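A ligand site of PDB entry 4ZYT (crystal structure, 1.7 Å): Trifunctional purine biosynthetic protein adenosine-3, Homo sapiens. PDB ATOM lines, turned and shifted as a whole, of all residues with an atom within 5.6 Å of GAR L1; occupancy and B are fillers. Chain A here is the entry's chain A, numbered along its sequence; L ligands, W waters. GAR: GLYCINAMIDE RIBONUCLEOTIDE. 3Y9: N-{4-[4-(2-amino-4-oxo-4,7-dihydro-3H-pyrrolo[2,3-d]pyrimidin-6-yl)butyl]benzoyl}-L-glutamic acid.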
ATOM      1  N   GLY A  10      18.722 -20.825 -13.897  1.00  0.00           N
ATOM      2  CA  GLY A  10      19.497 -20.083 -12.921  1.00  0.00           C
ATOM      3  C   GLY A  10      18.763 -19.224 -11.919  1.00  0.00           C
ATOM      4  O   GLY A  10      17.857 -19.689 -11.228  1.00  0.00           O
ATOM      5  N   THR A  11      19.157 -17.950 -11.849  1.00  0.00           N
ATOM      6  CA  THR A  11      18.737 -17.026 -10.807  1.00  0.00           C
ATOM      7  C   THR A  11      17.228 -16.833 -10.751  1.00  0.00           C
ATOM      8  O   THR A  11      16.621 -16.857  -9.682  1.00  0.00           O
ATOM      9  CB  THR A  11      19.414 -15.660 -10.998  1.00  0.00           C
ATOM     10  OG1 THR A  11      20.837 -15.817 -10.884  1.00  0.00           O
ATOM     11  CG2 THR A  11      18.926 -14.649  -9.957  1.00  0.00           C
ATOM     12  N   GLY A  12      16.620 -16.644 -11.926  1.00  0.00           N
ATOM     13  CA  GLY A  12      15.179 -16.531 -12.001  1.00  0.00           C
ATOM     14  C   GLY A  12      14.600 -15.153 -11.757  1.00  0.00           C
ATOM     15  O   GLY A  12      13.444 -15.040 -11.332  1.00  0.00           O
ATOM     16  N   SER A  13      15.349 -14.090 -12.052  1.00  0.00           N
ATOM     17  CA  SER A  13      14.758 -12.753 -11.960  1.00  0.00           C
ATOM     18  C   SER A  13      13.633 -12.566 -12.988  1.00  0.00           C
ATOM     19  O   SER A  13      12.626 -11.931 -12.680  1.00  0.00           O
ATOM     20  CB  SER A  13      15.821 -11.657 -12.122  1.00  0.00           C
ATOM     21  OG  SER A  13      16.263 -11.569 -13.467  1.00  0.00           O
ATOM     22  N   ASN A  14      13.788 -13.129 -14.183  1.00  0.00           N
ATOM     23  CA  ASN A  14      12.695 -13.040 -15.172  1.00  0.00           C
ATOM     24  C   ASN A  14      11.480 -13.837 -14.701  1.00  0.00           C
ATOM     25  O   ASN A  14      10.338 -13.382 -14.840  1.00  0.00           O
ATOM     26  CB  ASN A  14      13.157 -13.512 -16.556  1.00  0.00           C
ATOM     27  CG  ASN A  14      13.793 -12.384 -17.368  1.00  0.00           C
ATOM     28  OD1 ASN A  14      13.097 -11.489 -17.838  1.00  0.00           O
ATOM     29  ND2 ASN A  14      15.110 -12.434 -17.535  1.00  0.00           N
ATOM     30  N   LEU A  15      11.714 -15.013 -14.141  1.00  0.00           N
ATOM     31  CA  LEU A  15      10.638 -15.787 -13.539  1.00  0.00           C
ATOM     32  C   LEU A  15       9.878 -14.958 -12.486  1.00  0.00           C
ATOM     33  O   LEU A  15       8.653 -14.928 -12.487  1.00  0.00           O
ATOM     34  CB  LEU A  15      11.174 -17.062 -12.889  1.00  0.00           C
ATOM     35  CG  LEU A  15      10.187 -17.788 -11.960  1.00  0.00           C
ATOM     36  CD1 LEU A  15       8.949 -18.296 -12.720  1.00  0.00           C
ATOM     37  CD2 LEU A  15      10.889 -18.960 -11.236  1.00  0.00           C
ATOM     38  N   ALA A  87      12.984 -18.633 -19.633  1.00  0.00           N
ATOM     39  CA  ALA A  87      13.375 -17.470 -18.834  1.00  0.00           C
ATOM     40  C   ALA A  87      14.725 -17.753 -18.201  1.00  0.00           C
ATOM     41  O   ALA A  87      14.807 -18.230 -17.065  1.00  0.00           O
ATOM     42  CB  ALA A  87      12.312 -17.151 -17.780  1.00  0.00           C
ATOM     43  N   GLY A  88      15.790 -17.479 -18.958  1.00  0.00           N
ATOM     44  CA  GLY A  88      17.124 -17.854 -18.540  1.00  0.00           C
ATOM     45  C   GLY A  88      17.379 -19.341 -18.673  1.00  0.00           C
ATOM     46  O   GLY A  88      18.281 -19.881 -18.021  1.00  0.00           O
ATOM     47  N   PHE A  89      16.587 -20.020 -19.494  1.00  0.00           N
ATOM     48  CA  PHE A  89      16.791 -21.430 -19.814  1.00  0.00           C
ATOM     49  C   PHE A  89      17.872 -21.542 -20.877  1.00  0.00           C
ATOM     50  O   PHE A  89      17.677 -21.105 -22.016  1.00  0.00           O
ATOM     51  CB  PHE A  89      15.483 -22.047 -20.302  1.00  0.00           C
ATOM     52  CG  PHE A  89      15.553 -23.534 -20.525  1.00  0.00           C
ATOM     53  CD1 PHE A  89      15.553 -24.406 -19.446  1.00  0.00           C
ATOM     54  CD2 PHE A  89      15.567 -24.057 -21.808  1.00  0.00           C
ATOM     55  CE1 PHE A  89      15.592 -25.789 -19.662  1.00  0.00           C
ATOM     56  CE2 PHE A  89      15.603 -25.427 -22.025  1.00  0.00           C
ATOM     57  CZ  PHE A  89      15.613 -26.290 -20.949  1.00  0.00           C
ATOM     58  N   MET A  90      19.001 -22.137 -20.526  1.00  0.00           N
ATOM     59  CA  MET A  90      20.173 -22.084 -21.387  1.00  0.00           C
ATOM     60  C   MET A  90      20.464 -23.406 -22.079  1.00  0.00           C
ATOM     61  O   MET A  90      21.577 -23.931 -21.984  1.00  0.00           O
ATOM     62  CB  MET A  90      21.398 -21.627 -20.593  1.00  0.00           C
ATOM     63  CG  MET A  90      21.234 -20.245 -19.946  1.00  0.00           C
ATOM     64  SD  MET A  90      20.961 -18.921 -21.137  1.00  0.00           S
ATOM     65  CE  MET A  90      22.629 -18.626 -21.717  1.00  0.00           C
ATOM     66  N   ASN A 107      10.772 -16.818 -25.818  1.00  0.00           N
ATOM     67  CA  ASN A 107      12.116 -16.734 -25.215  1.00  0.00           C
ATOM     68  C   ASN A 107      12.504 -15.298 -24.979  1.00  0.00           C
ATOM     69  O   ASN A 107      12.132 -14.433 -25.775  1.00  0.00           O
ATOM     70  CB  ASN A 107      13.155 -17.404 -26.105  1.00  0.00           C
ATOM     71  CG  ASN A 107      14.554 -17.325 -25.524  1.00  0.00           C
ATOM     72  OD1 ASN A 107      14.805 -17.810 -24.405  1.00  0.00           O
ATOM     73  ND2 ASN A 107      15.491 -16.727 -26.264  1.00  0.00           N
ATOM     74  N   ILE A 108      13.236 -15.027 -23.901  1.00  0.00           N
ATOM     75  CA  ILE A 108      13.815 -13.689 -23.678  1.00  0.00           C
ATOM     76  C   ILE A 108      15.318 -13.762 -23.971  1.00  0.00           C
ATOM     77  O   ILE A 108      16.002 -14.712 -23.568  1.00  0.00           O
ATOM     78  CB  ILE A 108      13.562 -13.135 -22.232  1.00  0.00           C
ATOM     79  CG1 ILE A 108      14.160 -11.747 -22.056  1.00  0.00           C
ATOM     80  CG2 ILE A 108      14.150 -14.062 -21.174  1.00  0.00           C
ATOM     81  CD1 ILE A 108      13.314 -10.634 -22.572  1.00  0.00           C
ATOM     82  N   HIS A 109      15.802 -12.793 -24.725  1.00  0.00           N
ATOM     83  CA  HIS A 109      17.197 -12.775 -25.160  1.00  0.00           C
ATOM     84  C   HIS A 109      17.761 -11.386 -24.907  1.00  0.00           C
ATOM     85  O   HIS A 109      17.127 -10.392 -25.272  1.00  0.00           O
ATOM     86  CB  HIS A 109      17.304 -13.153 -26.636  1.00  0.00           C
ATOM     87  CG  HIS A 109      18.716 -13.175 -27.133  1.00  0.00           C
ATOM     88  ND1 HIS A 109      19.560 -14.240 -26.920  1.00  0.00           N
ATOM     89  CD2 HIS A 109      19.440 -12.237 -27.802  1.00  0.00           C
ATOM     90  CE1 HIS A 109      20.742 -13.974 -27.453  1.00  0.00           C
ATOM     91  NE2 HIS A 109      20.694 -12.770 -27.992  1.00  0.00           N
ATOM     92  N   PRO A 110      18.948 -11.305 -24.281  1.00  0.00           N
ATOM     93  CA  PRO A 110      19.455  -9.990 -23.858  1.00  0.00           C
ATOM     94  C   PRO A 110      20.255  -9.264 -24.948  1.00  0.00           C
ATOM     95  O   PRO A 110      21.358  -8.777 -24.706  1.00  0.00           O
ATOM     96  CB  PRO A 110      20.338 -10.334 -22.650  1.00  0.00           C
ATOM     97  CG  PRO A 110      20.911 -11.667 -23.006  1.00  0.00           C
ATOM     98  CD  PRO A 110      19.784 -12.403 -23.753  1.00  0.00           C
ATOM     99  N   GLY A 118      22.942 -15.963 -29.544  1.00  0.00           N
ATOM    100  CA  GLY A 118      23.735 -16.965 -28.851  1.00  0.00           C
ATOM    101  C   GLY A 118      23.805 -16.786 -27.348  1.00  0.00           C
ATOM    102  O   GLY A 118      23.047 -16.008 -26.775  1.00  0.00           O
ATOM    103  N   SER A 119      24.728 -17.497 -26.716  1.00  0.00           N
ATOM    104  CA  SER A 119      24.719 -17.616 -25.261  1.00  0.00           C
ATOM    105  C   SER A 119      25.423 -16.491 -24.507  1.00  0.00           C
ATOM    106  O   SER A 119      25.296 -16.401 -23.294  1.00  0.00           O
ATOM    107  CB  SER A 119      25.347 -18.949 -24.856  1.00  0.00           C
ATOM    108  OG  SER A 119      26.708 -18.962 -25.244  1.00  0.00           O
ATOM    109  N   HIS A 122      25.940 -10.265 -24.126  1.00  0.00           N
ATOM    110  CA  HIS A 122      26.552  -9.055 -23.546  1.00  0.00           C
ATOM    111  C   HIS A 122      28.032  -8.974 -23.905  1.00  0.00           C
ATOM    112  O   HIS A 122      28.545  -7.891 -24.213  1.00  0.00           O
ATOM    113  CB  HIS A 122      26.401  -9.023 -22.017  1.00  0.00           C
ATOM    114  CG  HIS A 122      24.982  -8.899 -21.563  1.00  0.00           C
ATOM    115  ND1 HIS A 122      24.153  -7.898 -22.001  1.00  0.00           N
ATOM    116  CD2 HIS A 122      24.248  -9.666 -20.722  1.00  0.00           C
ATOM    117  CE1 HIS A 122      22.959  -8.033 -21.443  1.00  0.00           C
ATOM    118  NE2 HIS A 122      22.988  -9.099 -20.666  1.00  0.00           N
ATOM    119  N   ASP A 145      17.405 -18.141 -31.769  1.00  0.00           N
ATOM    120  CA  ASP A 145      17.252 -16.687 -31.745  1.00  0.00           C
ATOM    121  C   ASP A 145      16.834 -16.101 -33.079  1.00  0.00           C
ATOM    122  O   ASP A 145      17.100 -14.932 -33.368  1.00  0.00           O
ATOM    123  CB  ASP A 145      18.560 -16.026 -31.257  1.00  0.00           C
ATOM    124  CG  ASP A 145      18.928 -16.438 -29.839  1.00  0.00           C
ATOM    125  OD1 ASP A 145      18.024 -16.859 -29.078  1.00  0.00           O
ATOM    126  OD2 ASP A 145      20.129 -16.347 -29.479  1.00  0.00           O
ATOM    127  N   LYS A 171      18.463  -6.279 -17.630  1.00  0.00           N
ATOM    128  CA  LYS A 171      17.426  -7.047 -16.917  1.00  0.00           C
ATOM    129  C   LYS A 171      16.241  -6.194 -16.466  1.00  0.00           C
ATOM    130  O   LYS A 171      15.117  -6.693 -16.377  1.00  0.00           O
ATOM    131  CB  LYS A 171      18.028  -7.789 -15.723  1.00  0.00           C
ATOM    132  CG  LYS A 171      18.717  -9.095 -16.128  1.00  0.00           C
ATOM    133  CD  LYS A 171      19.158  -9.892 -14.921  1.00  0.00           C
ATOM    134  CE  LYS A 171      19.904 -11.163 -15.324  1.00  0.00           C
ATOM    135  NZ  LYS A 171      20.233 -12.000 -14.120  1.00  0.00           N
ATOM    136  N   GLU A 174      14.143  -6.352 -19.424  1.00  0.00           N
ATOM    137  CA  GLU A 174      13.636  -7.707 -19.622  1.00  0.00           C
ATOM    138  C   GLU A 174      12.400  -7.922 -18.771  1.00  0.00           C
ATOM    139  O   GLU A 174      11.413  -8.527 -19.201  1.00  0.00           O
ATOM    140  CB  GLU A 174      14.689  -8.748 -19.261  1.00  0.00           C
ATOM    141  CG  GLU A 174      15.925  -8.756 -20.155  1.00  0.00           C
ATOM    142  CD  GLU A 174      16.912  -9.835 -19.746  1.00  0.00           C
ATOM    143  OE1 GLU A 174      16.468 -10.919 -19.314  1.00  0.00           O
ATOM    144  OE2 GLU A 174      18.127  -9.600 -19.830  1.00  0.00           O
ATOM    145  N   HIS A 175      12.459  -7.404 -17.549  1.00  0.00           N
ATOM    146  CA  HIS A 175      11.374  -7.595 -16.593  1.00  0.00           C
ATOM    147  C   HIS A 175      10.129  -6.802 -16.959  1.00  0.00           C
ATOM    148  O   HIS A 175       9.069  -7.021 -16.371  1.00  0.00           O
ATOM    149  CB  HIS A 175      11.831  -7.211 -15.197  1.00  0.00           C
ATOM    150  CG  HIS A 175      12.979  -8.027 -14.703  1.00  0.00           C
ATOM    151  ND1 HIS A 175      13.775  -7.627 -13.644  1.00  0.00           N
ATOM    152  CD2 HIS A 175      13.464  -9.219 -15.124  1.00  0.00           C
ATOM    153  CE1 HIS A 175      14.707  -8.544 -13.440  1.00  0.00           C
ATOM    154  NE2 HIS A 175      14.542  -9.521 -14.326  1.00  0.00           N
HETATM  155  C1  GAR L   1      18.570 -13.095 -18.725  1.00  0.00           C
HETATM  156  O6  GAR L   1      19.378 -11.936 -18.932  1.00  0.00           O
HETATM  157  C2  GAR L   1      18.169 -13.664 -20.062  1.00  0.00           C
HETATM  158  O8  GAR L   1      17.826 -12.672 -21.025  1.00  0.00           O
HETATM  159  C3  GAR L   1      19.426 -14.414 -20.457  1.00  0.00           C
HETATM  160  O4  GAR L   1      19.801 -15.058 -19.243  1.00  0.00           O
HETATM  161  C5  GAR L   1      19.432 -14.204 -18.147  1.00  0.00           C
HETATM  162  C10 GAR L   1      18.637 -14.995 -17.131  1.00  0.00           C
HETATM  163  O12 GAR L   1      18.505 -14.237 -15.927  1.00  0.00           O
HETATM  164  N19 GAR L   1      19.174 -15.358 -21.522  1.00  0.00           N
HETATM  165  C21 GAR L   1      20.074 -15.605 -22.456  1.00  0.00           C
HETATM  166  O22 GAR L   1      21.226 -15.159 -22.424  1.00  0.00           O
HETATM  167  C23 GAR L   1      19.583 -16.504 -23.567  1.00  0.00           C
HETATM  168  N24 GAR L   1      20.623 -16.790 -24.538  1.00  0.00           N
HETATM  169  P15 GAR L   1      17.411 -14.684 -14.825  1.00  0.00           P
HETATM  170  O16 GAR L   1      17.669 -13.709 -13.688  1.00  0.00           O
HETATM  171  O17 GAR L   1      17.723 -16.121 -14.483  1.00  0.00           O
HETATM  172  O18 GAR L   1      16.086 -14.548 -15.523  1.00  0.00           O
HETATM  173  C13 3Y9 L   2      23.236 -22.432 -26.775  1.00  0.00           C
HETATM  174  C15 3Y9 L   2      22.517 -21.255 -26.956  1.00  0.00           C
HETATM  175  C17 3Y9 L   2      24.092 -24.302 -25.222  1.00  0.00           C
HETATM  176  C20 3Y9 L   2      24.103 -26.301 -23.692  1.00  0.00           C
HETATM  177  C21 3Y9 L   2      23.895 -26.483 -22.209  1.00  0.00           C
HETATM  178  N1  3Y9 L   2      16.257 -23.444 -28.971  1.00  0.00           N
HETATM  179  C6  3Y9 L   2      16.974 -21.008 -26.435  1.00  0.00           C
HETATM  180  C7  3Y9 L   2      16.506 -20.312 -27.521  1.00  0.00           C
HETATM  181  C8  3Y9 L   2      16.169 -21.095 -28.618  1.00  0.00           C
HETATM  182  C9  3Y9 L   2      16.463 -22.392 -28.146  1.00  0.00           C
HETATM  183  C14 3Y9 L   2      22.711 -22.376 -24.422  1.00  0.00           C
HETATM  184  C16 3Y9 L   2      21.995 -21.214 -24.602  1.00  0.00           C
HETATM  185  C2  3Y9 L   2      15.784 -23.276 -30.209  1.00  0.00           C
HETATM  186  N3  3Y9 L   2      15.496 -22.051 -30.678  1.00  0.00           N
HETATM  187  C4  3Y9 L   2      15.675 -20.967 -29.911  1.00  0.00           C
HETATM  188  N5  3Y9 L   2      16.918 -22.271 -26.888  1.00  0.00           N
HETATM  189  O10 3Y9 L   2      15.403 -19.863 -30.394  1.00  0.00           O
HETATM  190  N11 3Y9 L   2      15.574 -24.398 -31.059  1.00  0.00           N
HETATM  191  C12 3Y9 L   2      23.342 -22.982 -25.496  1.00  0.00           C
HETATM  192  O18 3Y9 L   2      24.992 -24.700 -25.938  1.00  0.00           O
HETATM  193  N19 3Y9 L   2      23.601 -25.037 -24.109  1.00  0.00           N
HETATM  194  C22 3Y9 L   2      24.878 -25.668 -21.389  1.00  0.00           C
HETATM  195  C23 3Y9 L   2      24.818 -26.188 -19.960  1.00  0.00           C
HETATM  196  O24 3Y9 L   2      25.716 -25.864 -19.134  1.00  0.00           O
HETATM  197  O25 3Y9 L   2      23.873 -26.946 -19.609  1.00  0.00           O
HETATM  198  C26 3Y9 L   2      23.247 -27.343 -24.383  1.00  0.00           C
HETATM  199  O27 3Y9 L   2      22.272 -26.973 -25.097  1.00  0.00           O
HETATM  200  O28 3Y9 L   2      23.501 -28.568 -24.240  1.00  0.00           O
HETATM  201  C29 3Y9 L   2      17.453 -20.500 -25.085  1.00  0.00           C
HETATM  202  C30 3Y9 L   2      18.981 -20.469 -25.065  1.00  0.00           C
HETATM  203  C31 3Y9 L   2      19.562 -19.539 -26.117  1.00  0.00           C
HETATM  204  C32 3Y9 L   2      21.080 -19.392 -26.018  1.00  0.00           C
HETATM  205  C33 3Y9 L   2      21.898 -20.645 -25.861  1.00  0.00           C
HETATM  206  O   HOH W   1      20.271 -16.985 -14.444  1.00  0.00           O
HETATM  207  O   HOH W   2      14.196 -16.379 -14.964  1.00  0.00           O
HETATM  208  O   HOH W   3      16.516 -16.400 -21.535  1.00  0.00           O
HETATM  209  O   HOH W   4      22.088 -11.722 -18.817  1.00  0.00           O
HETATM  210  O   HOH W   5      23.070 -14.345 -24.465  1.00  0.00           O
HETATM  211  O   HOH W   6      21.943 -16.778 -18.160  1.00  0.00           O
HETATM  212  O   HOH W   7      18.452 -16.675 -26.461  1.00  0.00           O
HETATM  213  O   HOH W   8      16.975 -18.680 -15.210  1.00  0.00           O
HETATM  214  O   HOH W   9      20.575  -8.883 -19.179  1.00  0.00           O
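The backbone NH (N) of Ser 13 is in hydrogen-bond range of an oxygen (O16) of GAR L1 (2.9 Å). OG of Ser 13 is in hydrogen-bond range of O16 of GAR L1 (2.6 Å). The side-chain carboxylate of Glu 174 is in hydrogen-bond range of an oxygen (O6) of GAR L1. The backbone NH of Gly 12 sits at hydrogen-bond distance from an oxygen (O17) of GAR L1. N of Asn 14 lies within hydrogen-bond range of O18 of GAR L1, at 3.0 Å. The side-chain amide nitrogen (ND2) of Asn 14 sits at hydrogen-bond distance from an oxygen (O18) of GAR L1 (3.1 Å). The side-chain amino group of Lys 171 is in salt-bridge range of an oxygen (O16) of GAR L1 (3.1 Å). N24 of GAR L1 sits at hydrogen-bond distance from O of Gly 118. O of Met 90 sits close to N19 of 3Y9 L2 (3.1 Å). An oxygen (O10) of 3Y9 L2 sits at hydrogen-bond distance from the backbone NH of Asp 145 (3.0 Å).
NE2 of His 175 lies within hydrogen-bond range of OG of Ser 13 (2.8 Å). The side-chain carboxylate of Glu 174 lies within hydrogen-bond range of the side-chain amide nitrogen of Asn 14, 2.7 Å away. O of Lys 171 sits close to ND1 of His 175 (3.2 Å). N of Gly 118 sits at hydrogen-bond distance from OD2 of Asp 145 (2.8 Å). The side-chain carboxylate (OD2) of Asp 145 sits close to a ring nitrogen (ND1) of His 109.
Residues that only touch GAR L1: Pro 110, Thr 11, Gly 88, His 109, Met 90 and Ile 108. Hydrophobic or aromatic side chains within 4 Å of GAR L1: Met 90, Ile 108 and Pro 110. Of the 21 residues printed, 12 come within 4 Å of GAR L1. The nearest printed residue that does not touch GAR L1 is Gly 10 (4.2 Å).
Water W2 lies within hydrogen-bond range of O18 of GAR L1, O of Ala 87, N of Leu 15 and N of Asn 14. Water W1 lies within hydrogen-bond range of an oxygen (O17) of GAR L1 (2.7 Å) and the backbone NH of Thr 11 (3.0 Å). Water W4 bridges O6 of GAR L1 (2.7 Å) and NE2 of His 122 (3.3 Å). Water W3 lies within hydrogen-bond range of O of Ile 108 (2.7 Å), N19 of GAR L1 (2.9 Å) and N of Gly 88 (2.9 Å). Water W6 bridges O4 of GAR L1 and SD of Met 90. Water W9 lies within hydrogen-bond range of OE2 of Glu 174 (2.6 Å), NE2 of His 122 (2.8 Å) and O6 of GAR L1 (3.3 Å).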
